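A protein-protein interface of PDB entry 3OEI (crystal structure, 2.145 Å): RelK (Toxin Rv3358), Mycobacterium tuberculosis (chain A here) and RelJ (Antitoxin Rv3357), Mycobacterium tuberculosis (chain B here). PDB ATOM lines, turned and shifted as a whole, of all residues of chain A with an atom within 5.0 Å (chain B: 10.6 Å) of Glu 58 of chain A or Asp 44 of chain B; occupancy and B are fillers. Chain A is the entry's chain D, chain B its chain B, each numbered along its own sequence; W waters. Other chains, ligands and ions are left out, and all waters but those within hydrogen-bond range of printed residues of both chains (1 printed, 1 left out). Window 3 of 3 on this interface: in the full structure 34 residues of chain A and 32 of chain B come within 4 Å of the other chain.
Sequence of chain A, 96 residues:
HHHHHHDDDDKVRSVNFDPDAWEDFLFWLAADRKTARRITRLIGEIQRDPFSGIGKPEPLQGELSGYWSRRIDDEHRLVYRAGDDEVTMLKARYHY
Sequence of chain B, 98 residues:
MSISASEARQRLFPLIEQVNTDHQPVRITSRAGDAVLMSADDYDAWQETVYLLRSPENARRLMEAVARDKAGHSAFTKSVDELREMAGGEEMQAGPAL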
ATOM      1  N   LYS A  56     -18.412  38.456  -9.726  1.00  0.00           N
ATOM      2  CA  LYS A  56     -18.490  37.016  -9.939  1.00  0.00           C
ATOM      3  C   LYS A  56     -18.906  36.707 -11.360  1.00  0.00           C
ATOM      4  O   LYS A  56     -19.974  36.173 -11.580  1.00  0.00           O
ATOM      5  CB  LYS A  56     -19.502  36.371  -8.976  1.00  0.00           C
ATOM      6  CG  LYS A  56     -19.091  36.376  -7.509  1.00  0.00           C
ATOM      7  CD  LYS A  56     -20.027  35.516  -6.654  1.00  0.00           C
ATOM      8  CE  LYS A  56     -19.602  35.469  -5.171  1.00  0.00           C
ATOM      9  NZ  LYS A  56     -18.266  34.833  -4.921  1.00  0.00           N
ATOM     10  N   PRO A  57     -18.054  37.040 -12.333  1.00  0.00           N
ATOM     11  CA  PRO A  57     -18.440  36.841 -13.728  1.00  0.00           C
ATOM     12  C   PRO A  57     -18.673  35.354 -14.017  1.00  0.00           C
ATOM     13  O   PRO A  57     -17.863  34.532 -13.611  1.00  0.00           O
ATOM     14  CB  PRO A  57     -17.226  37.367 -14.507  1.00  0.00           C
ATOM     15  CG  PRO A  57     -16.397  38.124 -13.508  1.00  0.00           C
ATOM     16  CD  PRO A  57     -16.664  37.502 -12.192  1.00  0.00           C
ATOM     17  N   GLU A  58     -19.771  35.024 -14.699  1.00  0.00           N
ATOM     18  CA  GLU A  58     -20.147  33.632 -14.968  1.00  0.00           C
ATOM     19  C   GLU A  58     -20.404  33.449 -16.455  1.00  0.00           C
ATOM     20  O   GLU A  58     -21.104  34.271 -17.068  1.00  0.00           O
ATOM     21  CB  GLU A  58     -21.444  33.270 -14.233  1.00  0.00           C
ATOM     22  CG  GLU A  58     -21.346  33.179 -12.721  1.00  0.00           C
ATOM     23  CD  GLU A  58     -20.502  32.006 -12.264  1.00  0.00           C
ATOM     24  OE1 GLU A  58     -20.145  31.158 -13.120  1.00  0.00           O
ATOM     25  OE2 GLU A  58     -20.184  31.940 -11.053  1.00  0.00           O
ATOM     26  N   PRO A  59     -19.839  32.384 -17.051  1.00  0.00           N
ATOM     27  CA  PRO A  59     -20.233  32.026 -18.420  1.00  0.00           C
ATOM     28  C   PRO A  59     -21.609  31.381 -18.446  1.00  0.00           C
ATOM     29  O   PRO A  59     -21.833  30.327 -17.835  1.00  0.00           O
ATOM     30  CB  PRO A  59     -19.173  31.006 -18.841  1.00  0.00           C
ATOM     31  CG  PRO A  59     -18.693  30.404 -17.530  1.00  0.00           C
ATOM     32  CD  PRO A  59     -18.698  31.576 -16.576  1.00  0.00           C
ATOM     33  N   LEU A  60     -22.532  32.038 -19.137  1.00  0.00           N
ATOM     34  CA  LEU A  60     -23.881  31.530 -19.310  1.00  0.00           C
ATOM     35  C   LEU A  60     -23.864  30.329 -20.260  1.00  0.00           C
ATOM     36  O   LEU A  60     -23.024  30.251 -21.144  1.00  0.00           O
ATOM     37  CB  LEU A  60     -24.788  32.644 -19.834  1.00  0.00           C
ATOM     38  CG  LEU A  60     -25.550  33.540 -18.844  1.00  0.00           C
ATOM     39  CD1 LEU A  60     -25.046  33.492 -17.385  1.00  0.00           C
ATOM     40  CD2 LEU A  60     -25.628  34.972 -19.352  1.00  0.00           C
ATOM     41  N   TYR A  67     -22.595  34.261 -23.795  1.00  0.00           N
ATOM     42  CA  TYR A  67     -22.820  35.450 -23.002  1.00  0.00           C
ATOM     43  C   TYR A  67     -22.325  35.251 -21.573  1.00  0.00           C
ATOM     44  O   TYR A  67     -22.152  34.128 -21.101  1.00  0.00           O
ATOM     45  CB  TYR A  67     -24.301  35.820 -23.011  1.00  0.00           C
ATOM     46  CG  TYR A  67     -24.817  36.163 -24.394  1.00  0.00           C
ATOM     47  CD1 TYR A  67     -24.617  37.428 -24.938  1.00  0.00           C
ATOM     48  CD2 TYR A  67     -25.494  35.222 -25.156  1.00  0.00           C
ATOM     49  CE1 TYR A  67     -25.072  37.746 -26.206  1.00  0.00           C
ATOM     50  CE2 TYR A  67     -25.964  35.529 -26.419  1.00  0.00           C
ATOM     51  CZ  TYR A  67     -25.751  36.799 -26.943  1.00  0.00           C
ATOM     52  OH  TYR A  67     -26.208  37.100 -28.211  1.00  0.00           O
ATOM     53  N   TRP A  68     -22.107  36.361 -20.887  1.00  0.00           N
ATOM     54  CA  TRP A  68     -21.607  36.328 -19.532  1.00  0.00           C
ATOM     55  C   TRP A  68     -22.508  37.153 -18.634  1.00  0.00           C
ATOM     56  O   TRP A  68     -23.192  38.063 -19.094  1.00  0.00           O
ATOM     57  CB  TRP A  68     -20.169  36.879 -19.479  1.00  0.00           C
ATOM     58  CG  TRP A  68     -19.158  35.933 -20.014  1.00  0.00           C
ATOM     59  CD1 TRP A  68     -18.932  35.631 -21.328  1.00  0.00           C
ATOM     60  CD2 TRP A  68     -18.225  35.149 -19.252  1.00  0.00           C
ATOM     61  NE1 TRP A  68     -17.926  34.709 -21.429  1.00  0.00           N
ATOM     62  CE2 TRP A  68     -17.471  34.395 -20.174  1.00  0.00           C
ATOM     63  CE3 TRP A  68     -17.953  35.014 -17.886  1.00  0.00           C
ATOM     64  CZ2 TRP A  68     -16.463  33.519 -19.773  1.00  0.00           C
ATOM     65  CZ3 TRP A  68     -16.950  34.150 -17.488  1.00  0.00           C
ATOM     66  CH2 TRP A  68     -16.218  33.411 -18.427  1.00  0.00           C
ATOM     67  N   SER A  69     -22.476  36.851 -17.345  1.00  0.00           N
ATOM     68  CA  SER A  69     -23.214  37.633 -16.374  1.00  0.00           C
ATOM     69  C   SER A  69     -22.289  38.073 -15.252  1.00  0.00           C
ATOM     70  O   SER A  69     -21.458  37.303 -14.796  1.00  0.00           O
ATOM     71  CB  SER A  69     -24.337  36.789 -15.791  1.00  0.00           C
ATOM     72  OG  SER A  69     -24.943  37.439 -14.697  1.00  0.00           O
ATOM     73  N   ASN B  20     -13.383  18.662 -14.003  1.00  0.00           N
ATOM     74  CA  ASN B  20     -13.222  20.042 -14.434  1.00  0.00           C
ATOM     75  C   ASN B  20     -12.690  20.153 -15.861  1.00  0.00           C
ATOM     76  O   ASN B  20     -12.914  21.147 -16.529  1.00  0.00           O
ATOM     77  CB  ASN B  20     -12.271  20.791 -13.505  1.00  0.00           C
ATOM     78  CG  ASN B  20     -12.982  21.414 -12.307  1.00  0.00           C
ATOM     79  OD1 ASN B  20     -14.019  22.063 -12.448  1.00  0.00           O
ATOM     80  ND2 ASN B  20     -12.416  21.227 -11.128  1.00  0.00           N
ATOM     81  N   HIS B  23     -15.419  18.267 -18.191  1.00  0.00           N
ATOM     82  CA  HIS B  23     -16.765  18.764 -17.913  1.00  0.00           C
ATOM     83  C   HIS B  23     -17.770  17.618 -17.841  1.00  0.00           C
ATOM     84  O   HIS B  23     -18.844  17.687 -18.432  1.00  0.00           O
ATOM     85  CB  HIS B  23     -17.203  19.743 -19.005  1.00  0.00           C
ATOM     86  CG  HIS B  23     -16.356  20.973 -19.076  1.00  0.00           C
ATOM     87  ND1 HIS B  23     -16.651  22.121 -18.373  1.00  0.00           N
ATOM     88  CD2 HIS B  23     -15.207  21.225 -19.746  1.00  0.00           C
ATOM     89  CE1 HIS B  23     -15.729  23.034 -18.616  1.00  0.00           C
ATOM     90  NE2 HIS B  23     -14.839  22.514 -19.445  1.00  0.00           N
ATOM     91  N   MET B  38     -18.685  17.019  -9.258  1.00  0.00           N
ATOM     92  CA  MET B  38     -18.720  17.780 -10.504  1.00  0.00           C
ATOM     93  C   MET B  38     -17.949  19.062 -10.362  1.00  0.00           C
ATOM     94  O   MET B  38     -17.658  19.504  -9.255  1.00  0.00           O
ATOM     95  CB  MET B  38     -20.180  18.075 -10.921  1.00  0.00           C
ATOM     96  CG  MET B  38     -20.855  19.124 -10.040  1.00  0.00           C
ATOM     97  SD  MET B  38     -22.593  19.524 -10.475  1.00  0.00           S
ATOM     98  CE  MET B  38     -22.442  19.962 -12.218  1.00  0.00           C
ATOM     99  N   SER B  39     -17.627  19.657 -11.500  1.00  0.00           N
ATOM    100  CA  SER B  39     -17.039  20.991 -11.581  1.00  0.00           C
ATOM    101  C   SER B  39     -17.852  22.051 -10.843  1.00  0.00           C
ATOM    102  O   SER B  39     -19.021  22.245 -11.143  1.00  0.00           O
ATOM    103  CB  SER B  39     -16.926  21.403 -13.062  1.00  0.00           C
ATOM    104  OG  SER B  39     -16.601  22.774 -13.211  1.00  0.00           O
ATOM    105  N   ALA B  40     -17.218  22.749  -9.901  1.00  0.00           N
ATOM    106  CA  ALA B  40     -17.853  23.855  -9.212  1.00  0.00           C
ATOM    107  C   ALA B  40     -18.215  24.972 -10.207  1.00  0.00           C
ATOM    108  O   ALA B  40     -19.309  25.550 -10.126  1.00  0.00           O
ATOM    109  CB  ALA B  40     -16.941  24.397  -8.114  1.00  0.00           C
ATOM    110  N   ASP B  41     -17.309  25.281 -11.140  1.00  0.00           N
ATOM    111  CA  ASP B  41     -17.602  26.310 -12.155  1.00  0.00           C
ATOM    112  C   ASP B  41     -18.829  25.998 -13.017  1.00  0.00           C
ATOM    113  O   ASP B  41     -19.654  26.890 -13.263  1.00  0.00           O
ATOM    114  CB  ASP B  41     -16.400  26.605 -13.057  1.00  0.00           C
ATOM    115  CG  ASP B  41     -15.358  27.524 -12.384  1.00  0.00           C
ATOM    116  OD1 ASP B  41     -14.448  28.010 -13.100  1.00  0.00           O
ATOM    117  OD2 ASP B  41     -15.440  27.764 -11.149  1.00  0.00           O
ATOM    118  N   ASP B  42     -18.940  24.760 -13.495  1.00  0.00           N
ATOM    119  CA  ASP B  42     -20.114  24.364 -14.269  1.00  0.00           C
ATOM    120  C   ASP B  42     -21.374  24.418 -13.416  1.00  0.00           C
ATOM    121  O   ASP B  42     -22.414  24.888 -13.860  1.00  0.00           O
ATOM    122  CB  ASP B  42     -19.962  22.969 -14.884  1.00  0.00           C
ATOM    123  CG  ASP B  42     -18.845  22.901 -15.920  1.00  0.00           C
ATOM    124  OD1 ASP B  42     -18.398  23.957 -16.402  1.00  0.00           O
ATOM    125  OD2 ASP B  42     -18.407  21.783 -16.256  1.00  0.00           O
ATOM    126  N   TYR B  43     -21.283  23.932 -12.187  1.00  0.00           N
ATOM    127  CA  TYR B  43     -22.402  24.040 -11.269  1.00  0.00           C
ATOM    128  C   TYR B  43     -22.881  25.481 -11.115  1.00  0.00           C
ATOM    129  O   TYR B  43     -24.059  25.764 -11.329  1.00  0.00           O
ATOM    130  CB  TYR B  43     -22.053  23.440  -9.918  1.00  0.00           C
ATOM    131  CG  TYR B  43     -23.164  23.628  -8.931  1.00  0.00           C
ATOM    132  CD1 TYR B  43     -24.313  22.846  -9.001  1.00  0.00           C
ATOM    133  CD2 TYR B  43     -23.099  24.623  -7.974  1.00  0.00           C
ATOM    134  CE1 TYR B  43     -25.343  23.020  -8.118  1.00  0.00           C
ATOM    135  CE2 TYR B  43     -24.130  24.807  -7.073  1.00  0.00           C
ATOM    136  CZ  TYR B  43     -25.247  23.999  -7.151  1.00  0.00           C
ATOM    137  OH  TYR B  43     -26.273  24.169  -6.260  1.00  0.00           O
ATOM    138  N   ASP B  44     -21.962  26.392 -10.784  1.00  0.00           N
ATOM    139  CA  ASP B  44     -22.269  27.826 -10.647  1.00  0.00           C
ATOM    140  C   ASP B  44     -22.778  28.466 -11.937  1.00  0.00           C
ATOM    141  O   ASP B  44     -23.651  29.316 -11.903  1.00  0.00           O
ATOM    142  CB  ASP B  44     -21.050  28.632 -10.139  1.00  0.00           C
ATOM    143  CG  ASP B  44     -20.613  28.214  -8.739  1.00  0.00           C
ATOM    144  OD1 ASP B  44     -21.492  27.820  -7.940  1.00  0.00           O
ATOM    145  OD2 ASP B  44     -19.396  28.273  -8.435  1.00  0.00           O
ATOM    146  N   ALA B  45     -22.203  28.085 -13.069  1.00  0.00           N
ATOM    147  CA  ALA B  45     -22.580  28.702 -14.325  1.00  0.00           C
ATOM    148  C   ALA B  45     -24.010  28.295 -14.738  1.00  0.00           C
ATOM    149  O   ALA B  45     -24.751  29.098 -15.288  1.00  0.00           O
ATOM    150  CB  ALA B  45     -21.572  28.347 -15.419  1.00  0.00           C
ATOM    151  N   TRP B  46     -24.390  27.050 -14.464  1.00  0.00           N
ATOM    152  CA  TRP B  46     -25.751  26.606 -14.721  1.00  0.00           C
ATOM    153  C   TRP B  46     -26.763  27.233 -13.756  1.00  0.00           C
ATOM    154  O   TRP B  46     -27.876  27.596 -14.167  1.00  0.00           O
ATOM    155  CB  TRP B  46     -25.862  25.083 -14.664  1.00  0.00           C
ATOM    156  CG  TRP B  46     -25.498  24.435 -15.928  1.00  0.00           C
ATOM    157  CD1 TRP B  46     -24.406  23.647 -16.172  1.00  0.00           C
ATOM    158  CD2 TRP B  46     -26.218  24.523 -17.163  1.00  0.00           C
ATOM    159  NE1 TRP B  46     -24.410  23.237 -17.491  1.00  0.00           N
ATOM    160  CE2 TRP B  46     -25.514  23.763 -18.114  1.00  0.00           C
ATOM    161  CE3 TRP B  46     -27.388  25.181 -17.558  1.00  0.00           C
ATOM    162  CZ2 TRP B  46     -25.940  23.645 -19.437  1.00  0.00           C
ATOM    163  CZ3 TRP B  46     -27.813  25.049 -18.871  1.00  0.00           C
ATOM    164  CH2 TRP B  46     -27.089  24.285 -19.790  1.00  0.00           C
ATOM    165  N   GLN B  47     -26.401  27.336 -12.477  1.00  0.00           N
ATOM    166  CA  GLN B  47     -27.277  28.019 -11.521  1.00  0.00           C
ATOM    167  C   GLN B  47     -27.547  29.451 -11.994  1.00  0.00           C
ATOM    168  O   GLN B  47     -28.680  29.933 -11.940  1.00  0.00           O
ATOM    169  CB  GLN B  47     -26.699  28.037 -10.098  1.00  0.00           C
ATOM    170  CG  GLN B  47     -26.684  26.652  -9.387  1.00  0.00           C
ATOM    171  CD  GLN B  47     -28.091  26.098  -9.168  1.00  0.00           C
ATOM    172  OE1 GLN B  47     -28.704  25.577 -10.088  1.00  0.00           O
ATOM    173  NE2 GLN B  47     -28.601  26.218  -7.947  1.00  0.00           N
ATOM    174  N   GLU B  48     -26.507  30.126 -12.466  1.00  0.00           N
ATOM    175  CA  GLU B  48     -26.665  31.518 -12.866  1.00  0.00           C
ATOM    176  C   GLU B  48     -27.511  31.636 -14.152  1.00  0.00           C
ATOM    177  O   GLU B  48     -28.316  32.568 -14.303  1.00  0.00           O
ATOM    178  CB  GLU B  48     -25.308  32.206 -13.013  1.00  0.00           C
ATOM    179  CG  GLU B  48     -25.392  33.663 -13.502  1.00  0.00           C
ATOM    180  CD  GLU B  48     -26.123  34.599 -12.526  1.00  0.00           C
ATOM    181  OE1 GLU B  48     -26.243  34.277 -11.317  1.00  0.00           O
ATOM    182  OE2 GLU B  48     -26.581  35.668 -12.987  1.00  0.00           O
ATOM    183  N   THR B  49     -27.338  30.680 -15.060  1.00  0.00           N
ATOM    184  CA  THR B  49     -28.102  30.646 -16.298  1.00  0.00           C
ATOM    185  C   THR B  49     -29.585  30.507 -15.947  1.00  0.00           C
ATOM    186  O   THR B  49     -30.445  31.192 -16.470  1.00  0.00           O
ATOM    187  CB  THR B  49     -27.660  29.458 -17.168  1.00  0.00           C
ATOM    188  OG1 THR B  49     -26.294  29.634 -17.544  1.00  0.00           O
ATOM    189  CG2 THR B  49     -28.491  29.344 -18.424  1.00  0.00           C
ATOM    190  N   VAL B  50     -29.841  29.606 -15.019  1.00  0.00           N
ATOM    191  CA  VAL B  50     -31.160  29.234 -14.585  1.00  0.00           C
ATOM    192  C   VAL B  50     -31.795  30.348 -13.745  1.00  0.00           C
ATOM    193  O   VAL B  50     -33.008  30.563 -13.814  1.00  0.00           O
ATOM    194  CB  VAL B  50     -31.078  27.894 -13.830  1.00  0.00           C
ATOM    195  CG1 VAL B  50     -31.886  27.926 -12.537  1.00  0.00           C
ATOM    196  CG2 VAL B  50     -31.481  26.758 -14.752  1.00  0.00           C
ATOM    197  N   TYR B  51     -30.970  31.069 -12.981  1.00  0.00           N
ATOM    198  CA  TYR B  51     -31.434  32.266 -12.276  1.00  0.00           C
ATOM    199  C   TYR B  51     -32.020  33.302 -13.253  1.00  0.00           C
ATOM    200  O   TYR B  51     -33.067  33.884 -12.993  1.00  0.00           O
ATOM    201  CB  TYR B  51     -30.299  32.905 -11.447  1.00  0.00           C
ATOM    202  CG  TYR B  51     -30.681  34.242 -10.836  1.00  0.00           C
ATOM    203  CD1 TYR B  51     -31.569  34.303  -9.772  1.00  0.00           C
ATOM    204  CD2 TYR B  51     -30.176  35.433 -11.338  1.00  0.00           C
ATOM    205  CE1 TYR B  51     -31.929  35.492  -9.207  1.00  0.00           C
ATOM    206  CE2 TYR B  51     -30.537  36.655 -10.770  1.00  0.00           C
ATOM    207  CZ  TYR B  51     -31.425  36.670  -9.710  1.00  0.00           C
ATOM    208  OH  TYR B  51     -31.826  37.845  -9.124  1.00  0.00           O
ATOM    209  N   LEU B  52     -31.346  33.523 -14.381  1.00  0.00           N
ATOM    210  CA  LEU B  52     -31.825  34.487 -15.386  1.00  0.00           C
ATOM    211  C   LEU B  52     -33.135  34.097 -16.107  1.00  0.00           C
ATOM    212  O   LEU B  52     -33.922  34.963 -16.470  1.00  0.00           O
ATOM    213  CB  LEU B  52     -30.740  34.793 -16.422  1.00  0.00           C
ATOM    214  CG  LEU B  52     -29.524  35.539 -15.861  1.00  0.00           C
ATOM    215  CD1 LEU B  52     -28.343  35.456 -16.849  1.00  0.00           C
ATOM    216  CD2 LEU B  52     -29.858  36.996 -15.508  1.00  0.00           C
HETATM  217  O   HOH W   1     -18.337  29.428 -13.084  1.00  0.00           O
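The side-chain hydroxyl (OG) of Ser 69 of chain A sits at hydrogen-bond distance from the side-chain carboxylate (OE2) of Glu 48 of chain B, at 3.0 Å.
The backbone carbonyl oxygen (O) of Ala 45 of chain B is in hydrogen-bond range of the side-chain hydroxyl (OG1) of Thr 49 of chain B, at 2.8 Å.
N of Glu 58 of chain A lies within hydrogen-bond range of O of Ser 69 of chain A, 2.8 Å away.
O of Tyr 67 of chain A lies within hydrogen-bond range of N of Leu 60 of chain A, at 2.9 Å.
Among the printed residues, pairs that only touch across the chains: Pro 59 of chain A with Ala 45 of chain B, Glu 58 of chain A with Asp 44 of chain B, Leu 60 of chain A with Thr 49 of chain B, Glu 58 of chain A with Ala 45 of chain B, Leu 60 of chain A with Leu 52 of chain B and Leu 60 of chain A with Glu 48 of chain B.
Of chain B, only Asp 44 (3.5 Å) and Ala 45 (3.7 Å) come within 4 Å of Glu 58 of chain A.
Of chain A, only Glu 58 (3.5 Å) comes within 4 Å of Asp 44 of chain B.
No residue of chain B comes within 4 Å of Pro 57 of chain A.
Pro 59 of chain A touches just one residue of chain B: Ala 45.
No residue of chain B comes within 4 Å of Trp 68 of chain A.
Printed residues of chain A within 4 Å of Thr 49 of chain B: Leu 60.
Printed residues of chain A within 4 Å of Leu 52 of chain B: Leu 60 (3.7 Å).
Of the printed residues of chain A, Glu 48 of chain B touches Leu 60 and Ser 69.
Gln 47 of chain B touches none of the printed residues of chain A.
The nearest residue of chain B that does not touch Glu 58 of chain A is Glu 48 of chain B (4.03 Å).
The nearest printed residue of chain A that does not touch Asp 44 of chain B is Pro 59 of chain A (6.3 Å).
The nearest printed residue of chain A that does not touch Thr 49 of chain B is Pro 59 of chain A (4.5 Å).
Hydrophobic or aromatic side chains of chain B within 4 Å of the printed part of chain A: Ala 45 and Leu 52.
Of the 8 printed residues of chain A, 4 touch a printed residue of chain B.
Printed residues of chain A that touch a printed residue of chain B: Glu 58, Pro 59, Leu 60 and Ser 69.
Hydrophobic or aromatic side chains of chain A within 4 Å of the printed part of chain B: Leu 60.
Among the printed residues, no Asp or Glu carboxylate lies within 4 Å of a Lys or Arg side-chain nitrogen of the other chain.
Water W1 bridges the side-chain carboxylate (OE1) of Glu 58 of chain A (2.5 Å) and the backbone carbonyl oxygen (O) of Asp 41 of chain B (2.9 Å).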
